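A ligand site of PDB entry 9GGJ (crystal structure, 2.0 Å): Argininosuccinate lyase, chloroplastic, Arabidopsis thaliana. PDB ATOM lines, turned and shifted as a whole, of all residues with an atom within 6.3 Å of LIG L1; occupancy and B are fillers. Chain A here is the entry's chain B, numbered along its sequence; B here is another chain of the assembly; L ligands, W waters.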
ATOM      1  N   THR A  25     -10.803   0.205   2.847  1.00  0.00           N
ATOM      2  CA  THR A  25     -10.539  -0.711   3.953  1.00  0.00           C
ATOM      3  C   THR A  25     -10.911  -0.125   5.316  1.00  0.00           C
ATOM      4  O   THR A  25     -10.912  -0.882   6.298  1.00  0.00           O
ATOM      5  CB  THR A  25      -9.046  -1.048   3.927  1.00  0.00           C
ATOM      6  OG1 THR A  25      -8.390   0.189   4.175  1.00  0.00           O
ATOM      7  CG2 THR A  25      -8.657  -1.715   2.620  1.00  0.00           C
ATOM      8  N   SER A  27     -12.993   0.915   8.487  1.00  0.00           N
ATOM      9  CA  SER A  27     -14.162   0.311   9.096  1.00  0.00           C
ATOM     10  C   SER A  27     -14.831   1.238  10.125  1.00  0.00           C
ATOM     11  O   SER A  27     -15.922   0.918  10.627  1.00  0.00           O
ATOM     12  CB  SER A  27     -13.786  -1.022   9.722  1.00  0.00           C
ATOM     13  OG  SER A  27     -12.744  -0.792  10.662  1.00  0.00           O
ATOM     14  N   PHE A  30     -18.628   2.222  10.324  1.00  0.00           N
ATOM     15  CA  PHE A  30     -19.630   1.330  10.893  1.00  0.00           C
ATOM     16  C   PHE A  30     -19.218   0.791  12.269  1.00  0.00           C
ATOM     17  O   PHE A  30     -20.090   0.542  13.063  1.00  0.00           O
ATOM     18  CB  PHE A  30     -19.978   0.220   9.890  1.00  0.00           C
ATOM     19  CG  PHE A  30     -18.835  -0.677   9.409  1.00  0.00           C
ATOM     20  CD1 PHE A  30     -18.420  -1.777  10.153  1.00  0.00           C
ATOM     21  CD2 PHE A  30     -18.153  -0.376   8.232  1.00  0.00           C
ATOM     22  CE1 PHE A  30     -17.343  -2.556   9.727  1.00  0.00           C
ATOM     23  CE2 PHE A  30     -17.071  -1.142   7.824  1.00  0.00           C
ATOM     24  CZ  PHE A  30     -16.685  -2.250   8.553  1.00  0.00           C
ATOM     25  N   ASP A  31     -17.924   0.644  12.575  1.00  0.00           N
ATOM     26  CA  ASP A  31     -17.483  -0.090  13.758  1.00  0.00           C
ATOM     27  C   ASP A  31     -17.387   0.818  15.002  1.00  0.00           C
ATOM     28  O   ASP A  31     -17.126   0.369  16.120  1.00  0.00           O
ATOM     29  CB  ASP A  31     -16.230  -0.915  13.466  1.00  0.00           C
ATOM     30  CG  ASP A  31     -14.853  -0.223  13.547  1.00  0.00           C
ATOM     31  OD1 ASP A  31     -14.770   0.967  13.966  1.00  0.00           O
ATOM     32  OD2 ASP A  31     -13.840  -0.886  13.190  1.00  0.00           O
ATOM     33  N   ASP A  87     -10.093   2.484  12.419  1.00  0.00           N
ATOM     34  CA  ASP A  87     -11.096   1.683  13.097  1.00  0.00           C
ATOM     35  C   ASP A  87     -11.329   2.213  14.521  1.00  0.00           C
ATOM     36  O   ASP A  87     -10.649   3.143  14.979  1.00  0.00           O
ATOM     37  CB  ASP A  87     -10.737   0.196  13.021  1.00  0.00           C
ATOM     38  CG  ASP A  87      -9.453  -0.204  13.733  1.00  0.00           C
ATOM     39  OD1 ASP A  87      -9.061   0.500  14.672  1.00  0.00           O
ATOM     40  OD2 ASP A  87      -8.831  -1.201  13.315  1.00  0.00           O
ATOM     41  N   HIS A  89     -10.810   0.688  17.387  1.00  0.00           N
ATOM     42  CA  HIS A  89      -9.719   0.349  18.280  1.00  0.00           C
ATOM     43  C   HIS A  89      -8.627   1.428  18.246  1.00  0.00           C
ATOM     44  O   HIS A  89      -8.150   1.894  19.300  1.00  0.00           O
ATOM     45  CB  HIS A  89      -9.140  -1.032  17.930  1.00  0.00           C
ATOM     46  CG  HIS A  89     -10.155  -2.040  17.550  1.00  0.00           C
ATOM     47  ND1 HIS A  89     -11.050  -2.586  18.442  1.00  0.00           N
ATOM     48  CD2 HIS A  89     -10.478  -2.549  16.323  1.00  0.00           C
ATOM     49  CE1 HIS A  89     -11.855  -3.433  17.775  1.00  0.00           C
ATOM     50  NE2 HIS A  89     -11.526  -3.411  16.491  1.00  0.00           N
ATOM     51  N   SER A 112      -3.709  -8.215  20.444  1.00  0.00           N
ATOM     52  CA  SER A 112      -3.727  -7.974  19.008  1.00  0.00           C
ATOM     53  C   SER A 112      -5.095  -7.400  18.665  1.00  0.00           C
ATOM     54  O   SER A 112      -6.026  -7.553  19.440  1.00  0.00           O
ATOM     55  CB  SER A 112      -3.416  -9.259  18.264  1.00  0.00           C
ATOM     56  OG  SER A 112      -3.614  -9.119  16.879  1.00  0.00           O
ATOM     57  N   ARG A 113      -5.232  -6.761  17.503  1.00  0.00           N
ATOM     58  CA  ARG A 113      -6.578  -6.333  17.056  1.00  0.00           C
ATOM     59  C   ARG A 113      -7.392  -7.608  16.795  1.00  0.00           C
ATOM     60  O   ARG A 113      -8.589  -7.564  16.984  1.00  0.00           O
ATOM     61  CB  ARG A 113      -6.477  -5.449  15.815  1.00  0.00           C
ATOM     62  CG  ARG A 113      -5.710  -4.153  16.012  1.00  0.00           C
ATOM     63  CD  ARG A 113      -6.461  -3.127  16.833  1.00  0.00           C
ATOM     64  NE  ARG A 113      -5.753  -1.870  16.971  1.00  0.00           N
ATOM     65  CZ  ARG A 113      -5.299  -1.357  18.115  1.00  0.00           C
ATOM     66  NH1 ARG A 113      -5.500  -2.009  19.254  1.00  0.00           N
ATOM     67  NH2 ARG A 113      -4.665  -0.202  18.125  1.00  0.00           N
ATOM     68  N   ASN A 114      -6.720  -8.687  16.372  1.00  0.00           N
ATOM     69  CA  ASN A 114      -7.421  -9.941  16.086  1.00  0.00           C
ATOM     70  C   ASN A 114      -8.208 -10.452  17.299  1.00  0.00           C
ATOM     71  O   ASN A 114      -9.337 -10.894  17.154  1.00  0.00           O
ATOM     72  CB  ASN A 114      -6.438 -11.001  15.599  1.00  0.00           C
ATOM     73  CG  ASN A 114      -5.794 -10.669  14.271  1.00  0.00           C
ATOM     74  OD1 ASN A 114      -6.136  -9.669  13.640  1.00  0.00           O
ATOM     75  ND2 ASN A 114      -4.860 -11.503  13.840  1.00  0.00           N
ATOM     76  N   VAL A 117     -10.864  -7.405  18.534  1.00  0.00           N
ATOM     77  CA  VAL A 117     -12.123  -7.185  17.856  1.00  0.00           C
ATOM     78  C   VAL A 117     -13.085  -8.318  18.189  1.00  0.00           C
ATOM     79  O   VAL A 117     -14.278  -8.105  18.338  1.00  0.00           O
ATOM     80  CB  VAL A 117     -11.949  -6.982  16.335  1.00  0.00           C
ATOM     81  CG1 VAL A 117     -11.634  -8.256  15.571  1.00  0.00           C
ATOM     82  CG2 VAL A 117     -13.183  -6.309  15.743  1.00  0.00           C
ATOM     83  N   ARG A 236     -16.280 -17.177  13.834  1.00  0.00           N
ATOM     84  CA  ARG A 236     -17.429 -16.265  13.788  1.00  0.00           C
ATOM     85  C   ARG A 236     -18.749 -17.030  13.858  1.00  0.00           C
ATOM     86  O   ARG A 236     -19.775 -16.604  13.311  1.00  0.00           O
ATOM     87  CB  ARG A 236     -17.385 -15.435  12.492  1.00  0.00           C
ATOM     88  CG  ARG A 236     -16.174 -14.525  12.369  1.00  0.00           C
ATOM     89  CD  ARG A 236     -16.129 -13.477  13.496  1.00  0.00           C
ATOM     90  NE  ARG A 236     -15.040 -12.508  13.312  1.00  0.00           N
ATOM     91  CZ  ARG A 236     -13.818 -12.577  13.846  1.00  0.00           C
ATOM     92  NH1 ARG A 236     -13.479 -13.644  14.568  1.00  0.00           N
ATOM     93  NH2 ARG A 236     -12.955 -11.594  13.639  1.00  0.00           N
ATOM     94  N   TYR A 321      -6.829 -15.714  11.073  1.00  0.00           N
ATOM     95  CA  TYR A 321      -7.538 -14.457  10.842  1.00  0.00           C
ATOM     96  C   TYR A 321      -7.309 -14.084   9.374  1.00  0.00           C
ATOM     97  O   TYR A 321      -6.197 -14.228   8.859  1.00  0.00           O
ATOM     98  CB  TYR A 321      -7.127 -13.344  11.811  1.00  0.00           C
ATOM     99  CG  TYR A 321      -7.754 -12.004  11.466  1.00  0.00           C
ATOM    100  CD1 TYR A 321      -9.036 -11.671  11.880  1.00  0.00           C
ATOM    101  CD2 TYR A 321      -7.113 -11.100  10.625  1.00  0.00           C
ATOM    102  CE1 TYR A 321      -9.645 -10.470  11.521  1.00  0.00           C
ATOM    103  CE2 TYR A 321      -7.707  -9.918  10.237  1.00  0.00           C
ATOM    104  CZ  TYR A 321      -8.982  -9.590  10.686  1.00  0.00           C
ATOM    105  OH  TYR A 321      -9.578  -8.399  10.308  1.00  0.00           O
ATOM    106  N   ASN A 322      -8.399 -13.687   8.690  1.00  0.00           N
ATOM    107  CA  ASN A 322      -8.349 -13.067   7.376  1.00  0.00           C
ATOM    108  C   ASN A 322      -9.099 -11.731   7.415  1.00  0.00           C
ATOM    109  O   ASN A 322     -10.023 -11.541   8.203  1.00  0.00           O
ATOM    110  CB  ASN A 322      -8.941 -13.990   6.314  1.00  0.00           C
ATOM    111  CG  ASN A 322      -8.377 -15.389   6.366  1.00  0.00           C
ATOM    112  OD1 ASN A 322      -7.277 -15.632   5.845  1.00  0.00           O
ATOM    113  ND2 ASN A 322      -9.092 -16.309   7.009  1.00  0.00           N
ATOM    114  N   ARG A 323      -8.726 -10.804   6.528  1.00  0.00           N
ATOM    115  CA  ARG A 323      -9.299  -9.476   6.559  1.00  0.00           C
ATOM    116  C   ARG A 323     -10.744  -9.538   6.079  1.00  0.00           C
ATOM    117  O   ARG A 323     -11.489  -8.629   6.398  1.00  0.00           O
ATOM    118  CB  ARG A 323      -8.487  -8.468   5.751  1.00  0.00           C
ATOM    119  CG  ARG A 323      -8.823  -7.017   6.028  1.00  0.00           C
ATOM    120  CD  ARG A 323      -8.524  -6.571   7.475  1.00  0.00           C
ATOM    121  NE  ARG A 323      -8.859  -5.160   7.741  1.00  0.00           N
ATOM    122  CZ  ARG A 323      -8.203  -4.103   7.284  1.00  0.00           C
ATOM    123  NH1 ARG A 323      -7.078  -4.245   6.643  1.00  0.00           N
ATOM    124  NH2 ARG A 323      -8.686  -2.901   7.463  1.00  0.00           N
ATOM    125  N   PHE A 325     -13.064 -11.012   7.305  1.00  0.00           N
ATOM    126  CA  PHE A 325     -13.916 -11.042   8.480  1.00  0.00           C
ATOM    127  C   PHE A 325     -14.435  -9.661   8.914  1.00  0.00           C
ATOM    128  O   PHE A 325     -15.273  -9.575   9.819  1.00  0.00           O
ATOM    129  CB  PHE A 325     -13.172 -11.670   9.663  1.00  0.00           C
ATOM    130  CG  PHE A 325     -13.122 -13.190   9.653  1.00  0.00           C
ATOM    131  CD1 PHE A 325     -14.163 -13.939   9.108  1.00  0.00           C
ATOM    132  CD2 PHE A 325     -12.009 -13.852  10.161  1.00  0.00           C
ATOM    133  CE1 PHE A 325     -14.090 -15.325   9.084  1.00  0.00           C
ATOM    134  CE2 PHE A 325     -11.932 -15.227  10.118  1.00  0.00           C
ATOM    135  CZ  PHE A 325     -12.970 -15.960   9.577  1.00  0.00           C
ATOM    136  N   GLN A 326     -13.882  -8.567   8.351  1.00  0.00           N
ATOM    137  CA  GLN A 326     -14.369  -7.243   8.707  1.00  0.00           C
ATOM    138  C   GLN A 326     -15.786  -7.071   8.159  1.00  0.00           C
ATOM    139  O   GLN A 326     -16.506  -6.154   8.561  1.00  0.00           O
ATOM    140  CB  GLN A 326     -13.389  -6.263   8.083  1.00  0.00           C
ATOM    141  CG  GLN A 326     -13.720  -4.790   8.234  1.00  0.00           C
ATOM    142  CD  GLN A 326     -12.593  -3.880   7.800  1.00  0.00           C
ATOM    143  OE1 GLN A 326     -11.558  -3.760   8.464  1.00  0.00           O
ATOM    144  NE2 GLN A 326     -12.781  -3.245   6.664  1.00  0.00           N
ATOM    145  N   GLU A 327     -16.163  -7.932   7.203  1.00  0.00           N
ATOM    146  CA  GLU A 327     -17.467  -7.879   6.567  1.00  0.00           C
ATOM    147  C   GLU A 327     -18.538  -8.567   7.432  1.00  0.00           C
ATOM    148  O   GLU A 327     -19.665  -8.801   6.978  1.00  0.00           O
ATOM    149  CB  GLU A 327     -17.347  -8.505   5.167  1.00  0.00           C
ATOM    150  CG  GLU A 327     -16.508  -7.676   4.200  1.00  0.00           C
ATOM    151  CD  GLU A 327     -17.259  -6.399   3.838  1.00  0.00           C
ATOM    152  OE1 GLU A 327     -18.459  -6.598   3.527  1.00  0.00           O
ATOM    153  OE2 GLU A 327     -16.734  -5.247   3.915  1.00  0.00           O
ATOM    154  N   ASP A 328     -18.189  -8.927   8.673  1.00  0.00           N
ATOM    155  CA  ASP A 328     -19.139  -9.563   9.573  1.00  0.00           C
ATOM    156  C   ASP A 328     -19.919  -8.537  10.389  1.00  0.00           C
ATOM    157  O   ASP A 328     -20.950  -8.891  10.950  1.00  0.00           O
ATOM    158  CB  ASP A 328     -18.455 -10.558  10.497  1.00  0.00           C
ATOM    159  CG  ASP A 328     -17.471  -9.954  11.471  1.00  0.00           C
ATOM    160  OD1 ASP A 328     -17.240  -8.717  11.382  1.00  0.00           O
ATOM    161  OD2 ASP A 328     -16.901 -10.714  12.288  1.00  0.00           O
ATOM    162  N   LYS A 329     -19.459  -7.277  10.474  1.00  0.00           N
ATOM    163  CA  LYS A 329     -20.094  -6.357  11.417  1.00  0.00           C
ATOM    164  C   LYS A 329     -21.385  -5.799  10.818  1.00  0.00           C
ATOM    165  O   LYS A 329     -22.426  -5.840  11.465  1.00  0.00           O
ATOM    166  CB  LYS A 329     -19.336  -5.107  11.830  1.00  0.00           C
ATOM    167  CG  LYS A 329     -17.905  -5.257  12.205  1.00  0.00           C
ATOM    168  CD  LYS A 329     -17.660  -5.959  13.516  1.00  0.00           C
ATOM    169  CE  LYS A 329     -16.158  -5.953  13.592  1.00  0.00           C
ATOM    170  NZ  LYS A 329     -15.593  -7.002  12.719  1.00  0.00           N
ATOM    171  N   THR B 159      -1.898 -15.478   9.282  1.00  0.00           N
ATOM    172  CA  THR B 159      -2.907 -14.435   9.152  1.00  0.00           C
ATOM    173  C   THR B 159      -2.665 -13.741   7.815  1.00  0.00           C
ATOM    174  O   THR B 159      -1.513 -13.477   7.469  1.00  0.00           O
ATOM    175  CB  THR B 159      -2.876 -13.437  10.295  1.00  0.00           C
ATOM    176  OG1 THR B 159      -1.649 -12.723  10.142  1.00  0.00           O
ATOM    177  CG2 THR B 159      -3.030 -14.130  11.633  1.00  0.00           C
ATOM    178  N   HIS B 160      -3.795 -13.522   7.096  1.00  0.00           N
ATOM    179  CA  HIS B 160      -3.855 -13.023   5.725  1.00  0.00           C
ATOM    180  C   HIS B 160      -3.058 -13.927   4.789  1.00  0.00           C
ATOM    181  O   HIS B 160      -2.551 -13.465   3.768  1.00  0.00           O
ATOM    182  CB  HIS B 160      -3.330 -11.590   5.648  1.00  0.00           C
ATOM    183  CG  HIS B 160      -3.813 -10.622   6.683  1.00  0.00           C
ATOM    184  ND1 HIS B 160      -4.735  -9.631   6.419  1.00  0.00           N
ATOM    185  CD2 HIS B 160      -3.410 -10.438   7.969  1.00  0.00           C
ATOM    186  CE1 HIS B 160      -4.874  -8.881   7.517  1.00  0.00           C
ATOM    187  NE2 HIS B 160      -4.099  -9.380   8.477  1.00  0.00           N
HETATM  188  N1  LIG L   1     -11.174  -4.078  11.423  1.00  0.00           N
HETATM  189  C1  LIG L   1     -10.700  -5.456  11.725  1.00  0.00           C
HETATM  190  C2  LIG L   1     -11.893  -6.432  11.679  1.00  0.00           C
HETATM  191  O1  LIG L   1     -13.045  -5.921  11.780  1.00  0.00           O
HETATM  192  C3  LIG L   1     -10.006  -5.550  13.084  1.00  0.00           C
HETATM  193  C4  LIG L   1      -8.890  -6.580  13.158  1.00  0.00           C
HETATM  194  C5  LIG L   1      -7.679  -6.122  12.340  1.00  0.00           C
HETATM  195  N2  LIG L   1      -6.535  -7.035  12.416  1.00  0.00           N
HETATM  196  C6  LIG L   1      -5.242  -6.707  12.485  1.00  0.00           C
HETATM  197  N3  LIG L   1      -4.329  -7.635  12.205  1.00  0.00           N
HETATM  198  N4  LIG L   1      -4.833  -5.461  12.739  1.00  0.00           N
HETATM  199  O2  LIG L   1     -11.634  -7.657  11.540  1.00  0.00           O
HETATM  200  O1  LG2 L   2       1.891 -11.920  14.626  1.00  0.00           O
HETATM  201  C1  LG2 L   2       1.530 -11.397  13.552  1.00  0.00           C
HETATM  202  O2  LG2 L   2       2.293 -11.254  12.580  1.00  0.00           O
HETATM  203  C2  LG2 L   2       0.105 -10.820  13.480  1.00  0.00           C
HETATM  204  C3  LG2 L   2      -0.733 -10.753  12.427  1.00  0.00           C
HETATM  205  C4  LG2 L   2      -2.104 -10.088  12.347  1.00  0.00           C
HETATM  206  O3  LG2 L   2      -2.881 -10.358  11.412  1.00  0.00           O
HETATM  207  O4  LG2 L   2      -2.339  -9.233  13.180  1.00  0.00           O
HETATM  208  O   HOH W   1      -5.759  -6.304   9.487  1.00  0.00           O
HETATM  209  O   HOH W   2      -6.694  -3.555  10.314  1.00  0.00           O
HETATM  210  O   HOH W   3      -2.620  -7.321  10.492  1.00  0.00           O
HETATM  211  O   HOH W   4     -12.851  -3.408  14.194  1.00  0.00           O
HETATM  212  O   HOH W   5     -13.720  -9.185  12.208  1.00  0.00           O
HETATM  213  O   HOH W   6      -3.950  -2.236  12.395  1.00  0.00           O
HETATM  214  O   HOH W   7      -8.954  -2.543  10.940  1.00  0.00           O
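The side-chain hydroxyl of Tyr 321 sits at hydrogen-bond distance from an oxygen (O2) of LIG L1 (2.5 Å). NZ of Lys 329 lies within salt-bridge range of O1 of LIG L1 (2.9 Å). The side-chain amide oxygen of Asn 114 sits at hydrogen-bond distance from a nitrogen (N2) of LIG L1 (2.9 Å). A nitrogen (N1) of LIG L1 lies within hydrogen-bond range of the side-chain amide oxygen (OE1) of Gln 326. The side-chain amide nitrogen (ND2) of Asn 114 sits at hydrogen-bond distance from an oxygen (O3) of LG2 L2 (3.3 Å). A ring nitrogen (NE2) of His 160 of chain B is in hydrogen-bond range of an oxygen (O3) of LG2 L2 (3.3 Å). OG1 of Thr 159 of chain B lies within hydrogen-bond range of O3 of LG2 L2 (3.0 Å).
An oxygen (O4) of LG2 L2 is in hydrogen-bond range of a nitrogen (N3) of LIG L1 (2.7 Å).
Water W3 lies within hydrogen-bond range of N3 of LIG L1 (2.4 Å), O3 of LG2 L2 (3.2 Å) and NE2 of His 160 of chain B (3.2 Å). Water W5 lies within hydrogen-bond range of O2 of LIG L1 (2.7 Å), O of Phe 325 (2.9 Å), NH2 of Arg 236 (2.9 Å) and NZ of Lys 329 (2.9 Å). Water W7 bridges OD2 of Asp 87 (2.7 Å) and N1 of LIG L1 (2.7 Å). Water W4 lies within hydrogen-bond range of a ring nitrogen (NE2) of His 89, the side-chain carboxylate (OD2) of Asp 31 and a nitrogen (N1) of LIG L1.
Merely in contact with LIG L1: Ser 27, Arg 113 and Val 117. Of the 21 residues printed, 7 come within 4 Å of LIG L1. The nearest printed residue that does not touch LIG L1 is His 160 of chain B (4.1 Å).
The backbone carbonyl oxygen of Tyr 321 sits at hydrogen-bond distance from the backbone NH of His 160 of chain B, 3.1 Å away. The side-chain carboxylate (OD1) of Asp 328 is in salt-bridge range of the side-chain amino group (NZ) of Lys 329 (2.7 Å). The backbone NH (N) of Asn 114 lies close to the side-chain hydroxyl (OG) of Ser 112, at 3.2 Å. The side-chain amide oxygen of Gln 326 is in hydrogen-bond range of the guanidinium group of Arg 323, 3.1 Å away. The backbone carbonyl oxygen (O) of Thr 25 is in hydrogen-bond range of the side-chain amide nitrogen (NE2) of Gln 326. The side-chain hydroxyl of Ser 27 is in hydrogen-bond range of the side-chain carboxylate of Asp 31 (2.8 Å).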
